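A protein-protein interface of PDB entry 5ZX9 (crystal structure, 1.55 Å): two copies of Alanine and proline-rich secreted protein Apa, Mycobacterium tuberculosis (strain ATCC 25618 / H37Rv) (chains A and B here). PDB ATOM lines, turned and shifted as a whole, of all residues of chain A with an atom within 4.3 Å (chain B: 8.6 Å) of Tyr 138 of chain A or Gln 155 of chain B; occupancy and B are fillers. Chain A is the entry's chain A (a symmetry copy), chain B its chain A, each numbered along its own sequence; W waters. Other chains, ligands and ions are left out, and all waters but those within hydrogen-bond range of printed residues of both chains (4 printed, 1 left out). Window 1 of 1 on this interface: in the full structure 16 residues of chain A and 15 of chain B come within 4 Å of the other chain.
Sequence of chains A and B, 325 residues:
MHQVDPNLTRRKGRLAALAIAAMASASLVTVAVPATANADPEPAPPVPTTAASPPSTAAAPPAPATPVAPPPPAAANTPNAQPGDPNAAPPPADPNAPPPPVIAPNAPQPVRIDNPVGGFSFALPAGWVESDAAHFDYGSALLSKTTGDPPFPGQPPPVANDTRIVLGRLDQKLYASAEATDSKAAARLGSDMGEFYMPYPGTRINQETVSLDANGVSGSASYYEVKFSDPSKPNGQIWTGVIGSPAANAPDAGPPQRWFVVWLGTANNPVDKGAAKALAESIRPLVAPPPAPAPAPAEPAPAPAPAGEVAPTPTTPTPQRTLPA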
ATOM      1  N   VAL A 117      22.403 -14.114 -24.013  1.00  0.00           N
ATOM      2  CA  VAL A 117      22.690 -12.926 -23.203  1.00  0.00           C
ATOM      3  C   VAL A 117      21.438 -12.470 -22.461  1.00  0.00           C
ATOM      4  O   VAL A 117      21.512 -11.995 -21.316  1.00  0.00           O
ATOM      5  CB  VAL A 117      23.256 -11.800 -24.091  1.00  0.00           C
ATOM      6  CG1 VAL A 117      23.517 -10.534 -23.257  1.00  0.00           C
ATOM      7  CG2 VAL A 117      24.605 -12.254 -24.700  1.00  0.00           C
ATOM      8  N   ALA A 134      22.893  -8.124 -34.227  1.00  0.00           N
ATOM      9  CA  ALA A 134      23.563  -7.453 -33.110  1.00  0.00           C
ATOM     10  C   ALA A 134      22.645  -7.297 -31.924  1.00  0.00           C
ATOM     11  O   ALA A 134      23.144  -7.213 -30.783  1.00  0.00           O
ATOM     12  CB  ALA A 134      24.084  -6.090 -33.524  1.00  0.00           C
ATOM     13  N   HIS A 135      21.322  -7.354 -32.138  1.00  0.00           N
ATOM     14  CA  HIS A 135      20.437  -7.297 -30.971  1.00  0.00           C
ATOM     15  C   HIS A 135      20.775  -8.353 -29.937  1.00  0.00           C
ATOM     16  O   HIS A 135      20.682  -8.119 -28.715  1.00  0.00           O
ATOM     17  CB  HIS A 135      18.977  -7.481 -31.403  1.00  0.00           C
ATOM     18  CG  HIS A 135      18.343  -6.210 -31.863  1.00  0.00           C
ATOM     19  ND1 HIS A 135      18.636  -5.651 -33.095  1.00  0.00           N
ATOM     20  CD2 HIS A 135      17.425  -5.401 -31.265  1.00  0.00           C
ATOM     21  CE1 HIS A 135      17.964  -4.510 -33.210  1.00  0.00           C
ATOM     22  NE2 HIS A 135      17.234  -4.331 -32.122  1.00  0.00           N
ATOM     23  N   PHE A 136      21.146  -9.568 -30.396  1.00  0.00           N
ATOM     24  CA  PHE A 136      21.419 -10.611 -29.434  1.00  0.00           C
ATOM     25  C   PHE A 136      22.633 -10.333 -28.549  1.00  0.00           C
ATOM     26  O   PHE A 136      22.687 -10.909 -27.469  1.00  0.00           O
ATOM     27  CB  PHE A 136      21.620 -11.959 -30.202  1.00  0.00           C
ATOM     28  CG  PHE A 136      20.325 -12.649 -30.596  1.00  0.00           C
ATOM     29  CD1 PHE A 136      19.481 -12.110 -31.544  1.00  0.00           C
ATOM     30  CD2 PHE A 136      20.040 -13.866 -30.031  1.00  0.00           C
ATOM     31  CE1 PHE A 136      18.243 -12.762 -31.900  1.00  0.00           C
ATOM     32  CE2 PHE A 136      18.839 -14.530 -30.374  1.00  0.00           C
ATOM     33  CZ  PHE A 136      17.974 -13.981 -31.281  1.00  0.00           C
ATOM     34  N   ASP A 137      23.551  -9.454 -28.999  1.00  0.00           N
ATOM     35  CA  ASP A 137      24.769  -9.164 -28.232  1.00  0.00           C
ATOM     36  C   ASP A 137      24.403  -8.667 -26.849  1.00  0.00           C
ATOM     37  O   ASP A 137      25.168  -8.835 -25.903  1.00  0.00           O
ATOM     38  CB  ASP A 137      25.551  -8.068 -28.926  1.00  0.00           C
ATOM     39  CG  ASP A 137      26.167  -8.461 -30.207  1.00  0.00           C
ATOM     40  OD1 ASP A 137      26.210  -9.669 -30.516  1.00  0.00           O
ATOM     41  OD2 ASP A 137      26.648  -7.509 -30.878  1.00  0.00           O
ATOM     42  N   TYR A 138      23.245  -8.009 -26.721  1.00  0.00           N
ATOM     43  CA  TYR A 138      22.892  -7.359 -25.457  1.00  0.00           C
ATOM     44  C   TYR A 138      21.565  -7.847 -24.956  1.00  0.00           C
ATOM     45  O   TYR A 138      20.941  -7.201 -24.083  1.00  0.00           O
ATOM     46  CB  TYR A 138      22.919  -5.808 -25.594  1.00  0.00           C
ATOM     47  CG  TYR A 138      22.094  -5.264 -26.720  1.00  0.00           C
ATOM     48  CD1 TYR A 138      20.746  -4.978 -26.532  1.00  0.00           C
ATOM     49  CD2 TYR A 138      22.658  -5.006 -27.980  1.00  0.00           C
ATOM     50  CE1 TYR A 138      19.974  -4.482 -27.597  1.00  0.00           C
ATOM     51  CE2 TYR A 138      21.909  -4.468 -29.030  1.00  0.00           C
ATOM     52  CZ  TYR A 138      20.584  -4.205 -28.819  1.00  0.00           C
ATOM     53  OH  TYR A 138      19.858  -3.699 -29.871  1.00  0.00           O
ATOM     54  N   GLY A 139      21.090  -8.986 -25.458  1.00  0.00           N
ATOM     55  CA  GLY A 139      19.972  -9.672 -24.822  1.00  0.00           C
ATOM     56  C   GLY A 139      18.634  -9.362 -25.416  1.00  0.00           C
ATOM     57  O   GLY A 139      17.622  -9.660 -24.765  1.00  0.00           O
ATOM     58  N   SER A 140      18.585  -8.831 -26.646  1.00  0.00           N
ATOM     59  CA  SER A 140      17.324  -8.532 -27.335  1.00  0.00           C
ATOM     60  C   SER A 140      17.325  -9.237 -28.691  1.00  0.00           C
ATOM     61  O   SER A 140      18.312  -9.879 -29.095  1.00  0.00           O
ATOM     62  CB  SER A 140      17.100  -7.014 -27.523  1.00  0.00           C
ATOM     63  OG  SER A 140      16.788  -6.380 -26.296  1.00  0.00           O
ATOM     64  N   PHE A 196       8.355   6.182 -29.411  1.00  0.00           N
ATOM     65  CA  PHE A 196       9.615   5.876 -30.060  1.00  0.00           C
ATOM     66  C   PHE A 196       9.411   5.441 -31.512  1.00  0.00           C
ATOM     67  O   PHE A 196      10.245   5.744 -32.367  1.00  0.00           O
ATOM     68  CB  PHE A 196      10.275   4.713 -29.266  1.00  0.00           C
ATOM     69  CG  PHE A 196      11.697   4.429 -29.613  1.00  0.00           C
ATOM     70  CD1 PHE A 196      12.733   5.226 -29.138  1.00  0.00           C
ATOM     71  CD2 PHE A 196      12.004   3.272 -30.337  1.00  0.00           C
ATOM     72  CE1 PHE A 196      14.049   4.877 -29.399  1.00  0.00           C
ATOM     73  CE2 PHE A 196      13.341   2.914 -30.658  1.00  0.00           C
ATOM     74  CZ  PHE A 196      14.343   3.733 -30.175  1.00  0.00           C
ATOM     75  N   LEU B 124      29.423 -15.351 -18.963  1.00  0.00           N
ATOM     76  CA  LEU B 124      29.525 -13.898 -19.243  1.00  0.00           C
ATOM     77  C   LEU B 124      29.730 -13.129 -17.951  1.00  0.00           C
ATOM     78  O   LEU B 124      28.907 -13.277 -17.028  1.00  0.00           O
ATOM     79  CB  LEU B 124      28.202 -13.461 -19.930  1.00  0.00           C
ATOM     80  CG  LEU B 124      28.119 -11.997 -20.358  1.00  0.00           C
ATOM     81  CD1 LEU B 124      29.100 -11.685 -21.508  1.00  0.00           C
ATOM     82  CD2 LEU B 124      26.634 -11.764 -20.840  1.00  0.00           C
ATOM     83  N   TRP B 128      28.815  -7.017 -18.358  1.00  0.00           N
ATOM     84  CA  TRP B 128      29.363  -7.047 -19.722  1.00  0.00           C
ATOM     85  C   TRP B 128      28.367  -7.611 -20.717  1.00  0.00           C
ATOM     86  O   TRP B 128      27.480  -8.405 -20.349  1.00  0.00           O
ATOM     87  CB  TRP B 128      30.653  -7.896 -19.774  1.00  0.00           C
ATOM     88  CG  TRP B 128      31.750  -7.211 -18.938  1.00  0.00           C
ATOM     89  CD1 TRP B 128      31.816  -7.088 -17.571  1.00  0.00           C
ATOM     90  CD2 TRP B 128      32.939  -6.584 -19.463  1.00  0.00           C
ATOM     91  NE1 TRP B 128      32.977  -6.415 -17.218  1.00  0.00           N
ATOM     92  CE2 TRP B 128      33.682  -6.107 -18.361  1.00  0.00           C
ATOM     93  CE3 TRP B 128      33.440  -6.408 -20.751  1.00  0.00           C
ATOM     94  CZ2 TRP B 128      34.903  -5.422 -18.518  1.00  0.00           C
ATOM     95  CZ3 TRP B 128      34.671  -5.737 -20.927  1.00  0.00           C
ATOM     96  CH2 TRP B 128      35.385  -5.270 -19.796  1.00  0.00           C
ATOM     97  N   VAL B 129      28.484  -7.152 -21.959  1.00  0.00           N
ATOM     98  CA  VAL B 129      27.660  -7.646 -23.072  1.00  0.00           C
ATOM     99  C   VAL B 129      28.619  -8.043 -24.181  1.00  0.00           C
ATOM    100  O   VAL B 129      29.821  -7.725 -24.130  1.00  0.00           O
ATOM    101  CB  VAL B 129      26.649  -6.600 -23.625  1.00  0.00           C
ATOM    102  CG1 VAL B 129      25.549  -6.328 -22.572  1.00  0.00           C
ATOM    103  CG2 VAL B 129      27.370  -5.308 -23.977  1.00  0.00           C
ATOM    104  N   GLU B 130      28.120  -8.747 -25.191  1.00  0.00           N
ATOM    105  CA  GLU B 130      28.927  -9.004 -26.377  1.00  0.00           C
ATOM    106  C   GLU B 130      28.965  -7.777 -27.281  1.00  0.00           C
ATOM    107  O   GLU B 130      28.091  -6.903 -27.239  1.00  0.00           O
ATOM    108  CB  GLU B 130      28.361 -10.188 -27.175  1.00  0.00           C
ATOM    109  CG  GLU B 130      28.350 -11.473 -26.359  1.00  0.00           C
ATOM    110  CD  GLU B 130      27.577 -12.569 -27.041  1.00  0.00           C
ATOM    111  OE1 GLU B 130      26.875 -12.277 -28.026  1.00  0.00           O
ATOM    112  OE2 GLU B 130      27.586 -13.698 -26.549  1.00  0.00           O
ATOM    113  N   SER B 131      30.041  -7.665 -28.055  1.00  0.00           N
ATOM    114  CA  SER B 131      30.124  -6.651 -29.098  1.00  0.00           C
ATOM    115  C   SER B 131      30.626  -7.368 -30.349  1.00  0.00           C
ATOM    116  O   SER B 131      31.388  -8.344 -30.252  1.00  0.00           O
ATOM    117  CB  SER B 131      31.119  -5.560 -28.764  1.00  0.00           C
ATOM    118  OG  SER B 131      30.673  -4.863 -27.614  1.00  0.00           O
ATOM    119  N   ALA B 133      29.706  -9.262 -33.096  1.00  0.00           N
ATOM    120  CA  ALA B 133      29.378 -10.694 -33.124  1.00  0.00           C
ATOM    121  C   ALA B 133      30.076 -11.492 -34.228  1.00  0.00           C
ATOM    122  O   ALA B 133      30.111 -12.733 -34.126  1.00  0.00           O
ATOM    123  CB  ALA B 133      27.881 -10.854 -33.353  1.00  0.00           C
ATOM    124  N   SER B 144      32.203  -6.070 -24.101  1.00  0.00           N
ATOM    125  CA  SER B 144      32.313  -4.686 -23.671  1.00  0.00           C
ATOM    126  C   SER B 144      31.515  -4.465 -22.397  1.00  0.00           C
ATOM    127  O   SER B 144      30.564  -5.194 -22.078  1.00  0.00           O
ATOM    128  CB  SER B 144      31.741  -3.729 -24.708  1.00  0.00           C
ATOM    129  OG  SER B 144      32.456  -3.835 -25.948  1.00  0.00           O
ATOM    130  N   THR B 146      29.093  -2.380 -19.947  1.00  0.00           N
ATOM    131  CA  THR B 146      28.071  -1.339 -20.049  1.00  0.00           C
ATOM    132  C   THR B 146      28.320  -0.206 -19.078  1.00  0.00           C
ATOM    133  O   THR B 146      28.880  -0.399 -17.991  1.00  0.00           O
ATOM    134  CB  THR B 146      26.653  -1.916 -19.834  1.00  0.00           C
ATOM    135  OG1 THR B 146      26.531  -2.455 -18.517  1.00  0.00           O
ATOM    136  CG2 THR B 146      26.357  -2.997 -20.864  1.00  0.00           C
ATOM    137  N   ASP B 149      22.984   4.532 -17.486  1.00  0.00           N
ATOM    138  CA  ASP B 149      21.686   3.961 -17.213  1.00  0.00           C
ATOM    139  C   ASP B 149      21.333   3.011 -18.346  1.00  0.00           C
ATOM    140  O   ASP B 149      21.921   3.095 -19.417  1.00  0.00           O
ATOM    141  CB  ASP B 149      20.649   5.069 -17.082  1.00  0.00           C
ATOM    142  CG  ASP B 149      20.851   5.903 -15.822  1.00  0.00           C
ATOM    143  OD1 ASP B 149      21.040   5.293 -14.738  1.00  0.00           O
ATOM    144  OD2 ASP B 149      20.836   7.155 -15.925  1.00  0.00           O
ATOM    145  N   PRO B 150      20.405   2.086 -18.123  1.00  0.00           N
ATOM    146  CA  PRO B 150      19.992   1.206 -19.216  1.00  0.00           C
ATOM    147  C   PRO B 150      19.497   2.013 -20.395  1.00  0.00           C
ATOM    148  O   PRO B 150      18.873   3.080 -20.241  1.00  0.00           O
ATOM    149  CB  PRO B 150      18.870   0.359 -18.587  1.00  0.00           C
ATOM    150  CG  PRO B 150      19.146   0.386 -17.083  1.00  0.00           C
ATOM    151  CD  PRO B 150      19.711   1.773 -16.853  1.00  0.00           C
ATOM    152  N   PRO B 151      19.739   1.526 -21.609  1.00  0.00           N
ATOM    153  CA  PRO B 151      19.215   2.150 -22.821  1.00  0.00           C
ATOM    154  C   PRO B 151      17.707   1.858 -22.952  1.00  0.00           C
ATOM    155  O   PRO B 151      17.121   1.089 -22.177  1.00  0.00           O
ATOM    156  CB  PRO B 151      20.019   1.401 -23.906  1.00  0.00           C
ATOM    157  CG  PRO B 151      20.204   0.025 -23.293  1.00  0.00           C
ATOM    158  CD  PRO B 151      20.555   0.347 -21.851  1.00  0.00           C
ATOM    159  N   PHE B 152      17.095   2.504 -23.938  1.00  0.00           N
ATOM    160  CA  PHE B 152      15.700   2.210 -24.263  1.00  0.00           C
ATOM    161  C   PHE B 152      15.587   0.715 -24.571  1.00  0.00           C
ATOM    162  O   PHE B 152      16.455   0.179 -25.243  1.00  0.00           O
ATOM    163  CB  PHE B 152      15.217   3.026 -25.468  1.00  0.00           C
ATOM    164  CG  PHE B 152      13.742   3.000 -25.635  1.00  0.00           C
ATOM    165  CD1 PHE B 152      12.925   3.628 -24.728  1.00  0.00           C
ATOM    166  CD2 PHE B 152      13.197   2.332 -26.724  1.00  0.00           C
ATOM    167  CE1 PHE B 152      11.501   3.573 -24.874  1.00  0.00           C
ATOM    168  CE2 PHE B 152      11.799   2.297 -26.886  1.00  0.00           C
ATOM    169  CZ  PHE B 152      10.968   2.906 -26.011  1.00  0.00           C
ATOM    170  N   PRO B 153      14.514   0.031 -24.139  1.00  0.00           N
ATOM    171  CA  PRO B 153      14.468  -1.434 -24.359  1.00  0.00           C
ATOM    172  C   PRO B 153      14.596  -1.780 -25.835  1.00  0.00           C
ATOM    173  O   PRO B 153      13.903  -1.226 -26.684  1.00  0.00           O
ATOM    174  CB  PRO B 153      13.095  -1.846 -23.787  1.00  0.00           C
ATOM    175  CG  PRO B 153      12.972  -0.844 -22.612  1.00  0.00           C
ATOM    176  CD  PRO B 153      13.436   0.492 -23.259  1.00  0.00           C
ATOM    177  N   GLY B 154      15.478  -2.764 -26.132  1.00  0.00           N
ATOM    178  CA  GLY B 154      15.718  -3.166 -27.504  1.00  0.00           C
ATOM    179  C   GLY B 154      16.894  -2.480 -28.132  1.00  0.00           C
ATOM    180  O   GLY B 154      17.337  -2.895 -29.203  1.00  0.00           O
ATOM    181  N   GLN B 155      17.376  -1.377 -27.498  1.00  0.00           N
ATOM    182  CA  GLN B 155      18.493  -0.631 -28.052  1.00  0.00           C
ATOM    183  C   GLN B 155      19.800  -0.988 -27.371  1.00  0.00           C
ATOM    184  O   GLN B 155      19.800  -1.445 -26.229  1.00  0.00           O
ATOM    185  CB  GLN B 155      18.214   0.874 -27.838  1.00  0.00           C
ATOM    186  CG  GLN B 155      16.969   1.413 -28.581  1.00  0.00           C
ATOM    187  CD  GLN B 155      17.123   1.314 -30.055  1.00  0.00           C
ATOM    188  OE1 GLN B 155      18.082   1.874 -30.627  1.00  0.00           O
ATOM    189  NE2 GLN B 155      16.253   0.566 -30.691  1.00  0.00           N
ATOM    190  N   PRO B 156      20.944  -0.804 -28.044  1.00  0.00           N
ATOM    191  CA  PRO B 156      22.208  -1.250 -27.468  1.00  0.00           C
ATOM    192  C   PRO B 156      22.623  -0.353 -26.332  1.00  0.00           C
ATOM    193  O   PRO B 156      22.458   0.878 -26.403  1.00  0.00           O
ATOM    194  CB  PRO B 156      23.180  -1.147 -28.654  1.00  0.00           C
ATOM    195  CG  PRO B 156      22.506  -0.262 -29.667  1.00  0.00           C
ATOM    196  CD  PRO B 156      21.009  -0.358 -29.437  1.00  0.00           C
ATOM    197  N   PRO B 157      23.205  -0.929 -25.293  1.00  0.00           N
ATOM    198  CA  PRO B 157      23.657  -0.120 -24.144  1.00  0.00           C
ATOM    199  C   PRO B 157      24.930   0.615 -24.491  1.00  0.00           C
ATOM    200  O   PRO B 157      25.779   0.104 -25.230  1.00  0.00           O
ATOM    201  CB  PRO B 157      23.889  -1.167 -23.044  1.00  0.00           C
ATOM    202  CG  PRO B 157      24.330  -2.428 -23.863  1.00  0.00           C
ATOM    203  CD  PRO B 157      23.376  -2.394 -25.053  1.00  0.00           C
ATOM    204  N   PRO B 158      25.090   1.829 -23.985  1.00  0.00           N
ATOM    205  CA  PRO B 158      26.419   2.459 -24.018  1.00  0.00           C
ATOM    206  C   PRO B 158      27.445   1.553 -23.342  1.00  0.00           C
ATOM    207  O   PRO B 158      27.148   0.922 -22.336  1.00  0.00           O
ATOM    208  CB  PRO B 158      26.210   3.742 -23.214  1.00  0.00           C
ATOM    209  CG  PRO B 158      24.741   4.002 -23.201  1.00  0.00           C
ATOM    210  CD  PRO B 158      24.093   2.614 -23.245  1.00  0.00           C
ATOM    211  N   VAL B 159      28.671   1.565 -23.887  1.00  0.00           N
ATOM    212  CA  VAL B 159      29.739   0.775 -23.274  1.00  0.00           C
ATOM    213  C   VAL B 159      30.954   1.640 -23.082  1.00  0.00           C
ATOM    214  O   VAL B 159      31.145   2.666 -23.738  1.00  0.00           O
ATOM    215  CB  VAL B 159      30.111  -0.492 -24.079  1.00  0.00           C
ATOM    216  CG1 VAL B 159      28.872  -1.458 -24.105  1.00  0.00           C
ATOM    217  CG2 VAL B 159      30.526  -0.154 -25.504  1.00  0.00           C
HETATM  218  O   HOH W   1      28.750 -11.659 -30.154  1.00  0.00           O
HETATM  219  O   HOH W   2      15.322  -2.494 -31.657  1.00  0.00           O
HETATM  220  O   HOH W   3      25.226 -12.350 -30.513  1.00  0.00           O
HETATM  221  O   HOH W   4      27.518  -7.380 -33.369  1.00  0.00           O
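Hydrophobic or aromatic side chains of chain A that line the printed part of chain B: Val 117, His 135, Tyr 138 and Phe 196. Among the printed residues, no Asp or Glu carboxylate lies within 4 Å of a Lys or Arg side-chain nitrogen of the other chain.
N of Glu 130 of chain B lies within hydrogen-bond range of O of Asp 137 of chain A, at 3.0 Å. O of Gly 154 of chain B sits close to NE2 of His 135 of chain A, 3.3 Å away. O of Gly 154 of chain B sits at hydrogen-bond distance from OH of Tyr 138 of chain A (2.7 Å).
No position is printed for both chains. Of the 13 pairs that touch across the chains among the printed residues, none has its exchanged pair printed and touching as well.
Water W4 bridges OD2 of Asp 137 of chain A (2.6 Å) and N of Ala 133 of chain B (2.9 Å). Water W2 lies within hydrogen-bond range of NE2 of His 135 of chain A (2.7 Å), O of Gly 154 of chain B (3.2 Å) and NE2 of Gln 155 of chain B (3.3 Å). Water W3 lies within hydrogen-bond range of the side-chain carboxylate (OD1) of Asp 137 of chain A (2.9 Å) and the side-chain carboxylate (OE1) of Glu 130 of chain B (3.0 Å). Water W1 bridges OE1 of Glu 130 of chain B (2.9 Å) and OD1 of Asp 137 of chain A (3.2 Å).
CG2 of Val 117 of chain A touches OE2 of Glu 130 of chain B (3.8 Å). Asp 137 of chain A touches Val 129 of chain B (O to CB, 3.5 Å). OD2 of Asp 137 of chain A touches CA of Ser 131 of chain B, at 3.998 Å. Asp 137 of chain A touches Ala 133 of chain B (OD1 to CB, 3.5 Å). CE1 of Tyr 138 of chain A touches O of Gln 155 of chain B, 3.3 Å away. Pro 156 of chain B touches Tyr 138 of chain A. Tyr 138 of chain A touches Pro 157 of chain B (CB to CD, 3.5 Å). CA of Gly 154 of chain B touches OG of Ser 140 of chain A, at 3.6 Å. Phe 152 of chain B touches Phe 196 of chain A (CE2 to CG, 3.5 Å). Gln 155 of chain B touches Phe 196 of chain A.
Of chain B, only Gly 154 (2.7 Å), Gln 155 (3.3 Å), Pro 156 (3.5 Å) and Pro 157 (3.5 Å) come within 4 Å of Tyr 138 of chain A. Gln 155 of chain B touches just these residues of chain A: Tyr 138 (3.3 Å) and Phe 196 (3.7 Å). Of chain B, only Gly 154 (3.2 Å) comes within 4 Å of His 135 of chain A. No residue of chain B comes within 4 Å of Gly 139 of chain A. Of the printed residues of chain B, Asp 137 of chain A touches Val 129 (3.5 Å), Glu 130 (3.0 Å), Ser 131 (3.998 Å) and Ala 133 (3.5 Å). Of the printed residues of chain B, Ser 140 of chain A touches Gly 154. The nearest residue of chain B that does not touch Tyr 138 of chain A is Val 129 of chain B (4.04 Å). The nearest printed residue of chain A that does not touch Gln 155 of chain B is Ser 140 of chain A (5.2 Å). The nearest printed residue of chain B that does not touch Phe 196 of chain A is Pro 153 of chain B (5.8 Å).
The backbone NH (N) of Val 129 of chain B sits at hydrogen-bond distance from the backbone carbonyl oxygen (O) of Ser 144 of chain B (2.9 Å). The side-chain hydroxyl (OG) of Ser 144 of chain B is in hydrogen-bond range of the side-chain hydroxyl (OG) of Ser 131 of chain B (2.6 Å). The backbone NH (N) of Ser 140 of chain A lies within hydrogen-bond range of the backbone carbonyl oxygen (O) of His 135 of chain A (3.0 Å).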
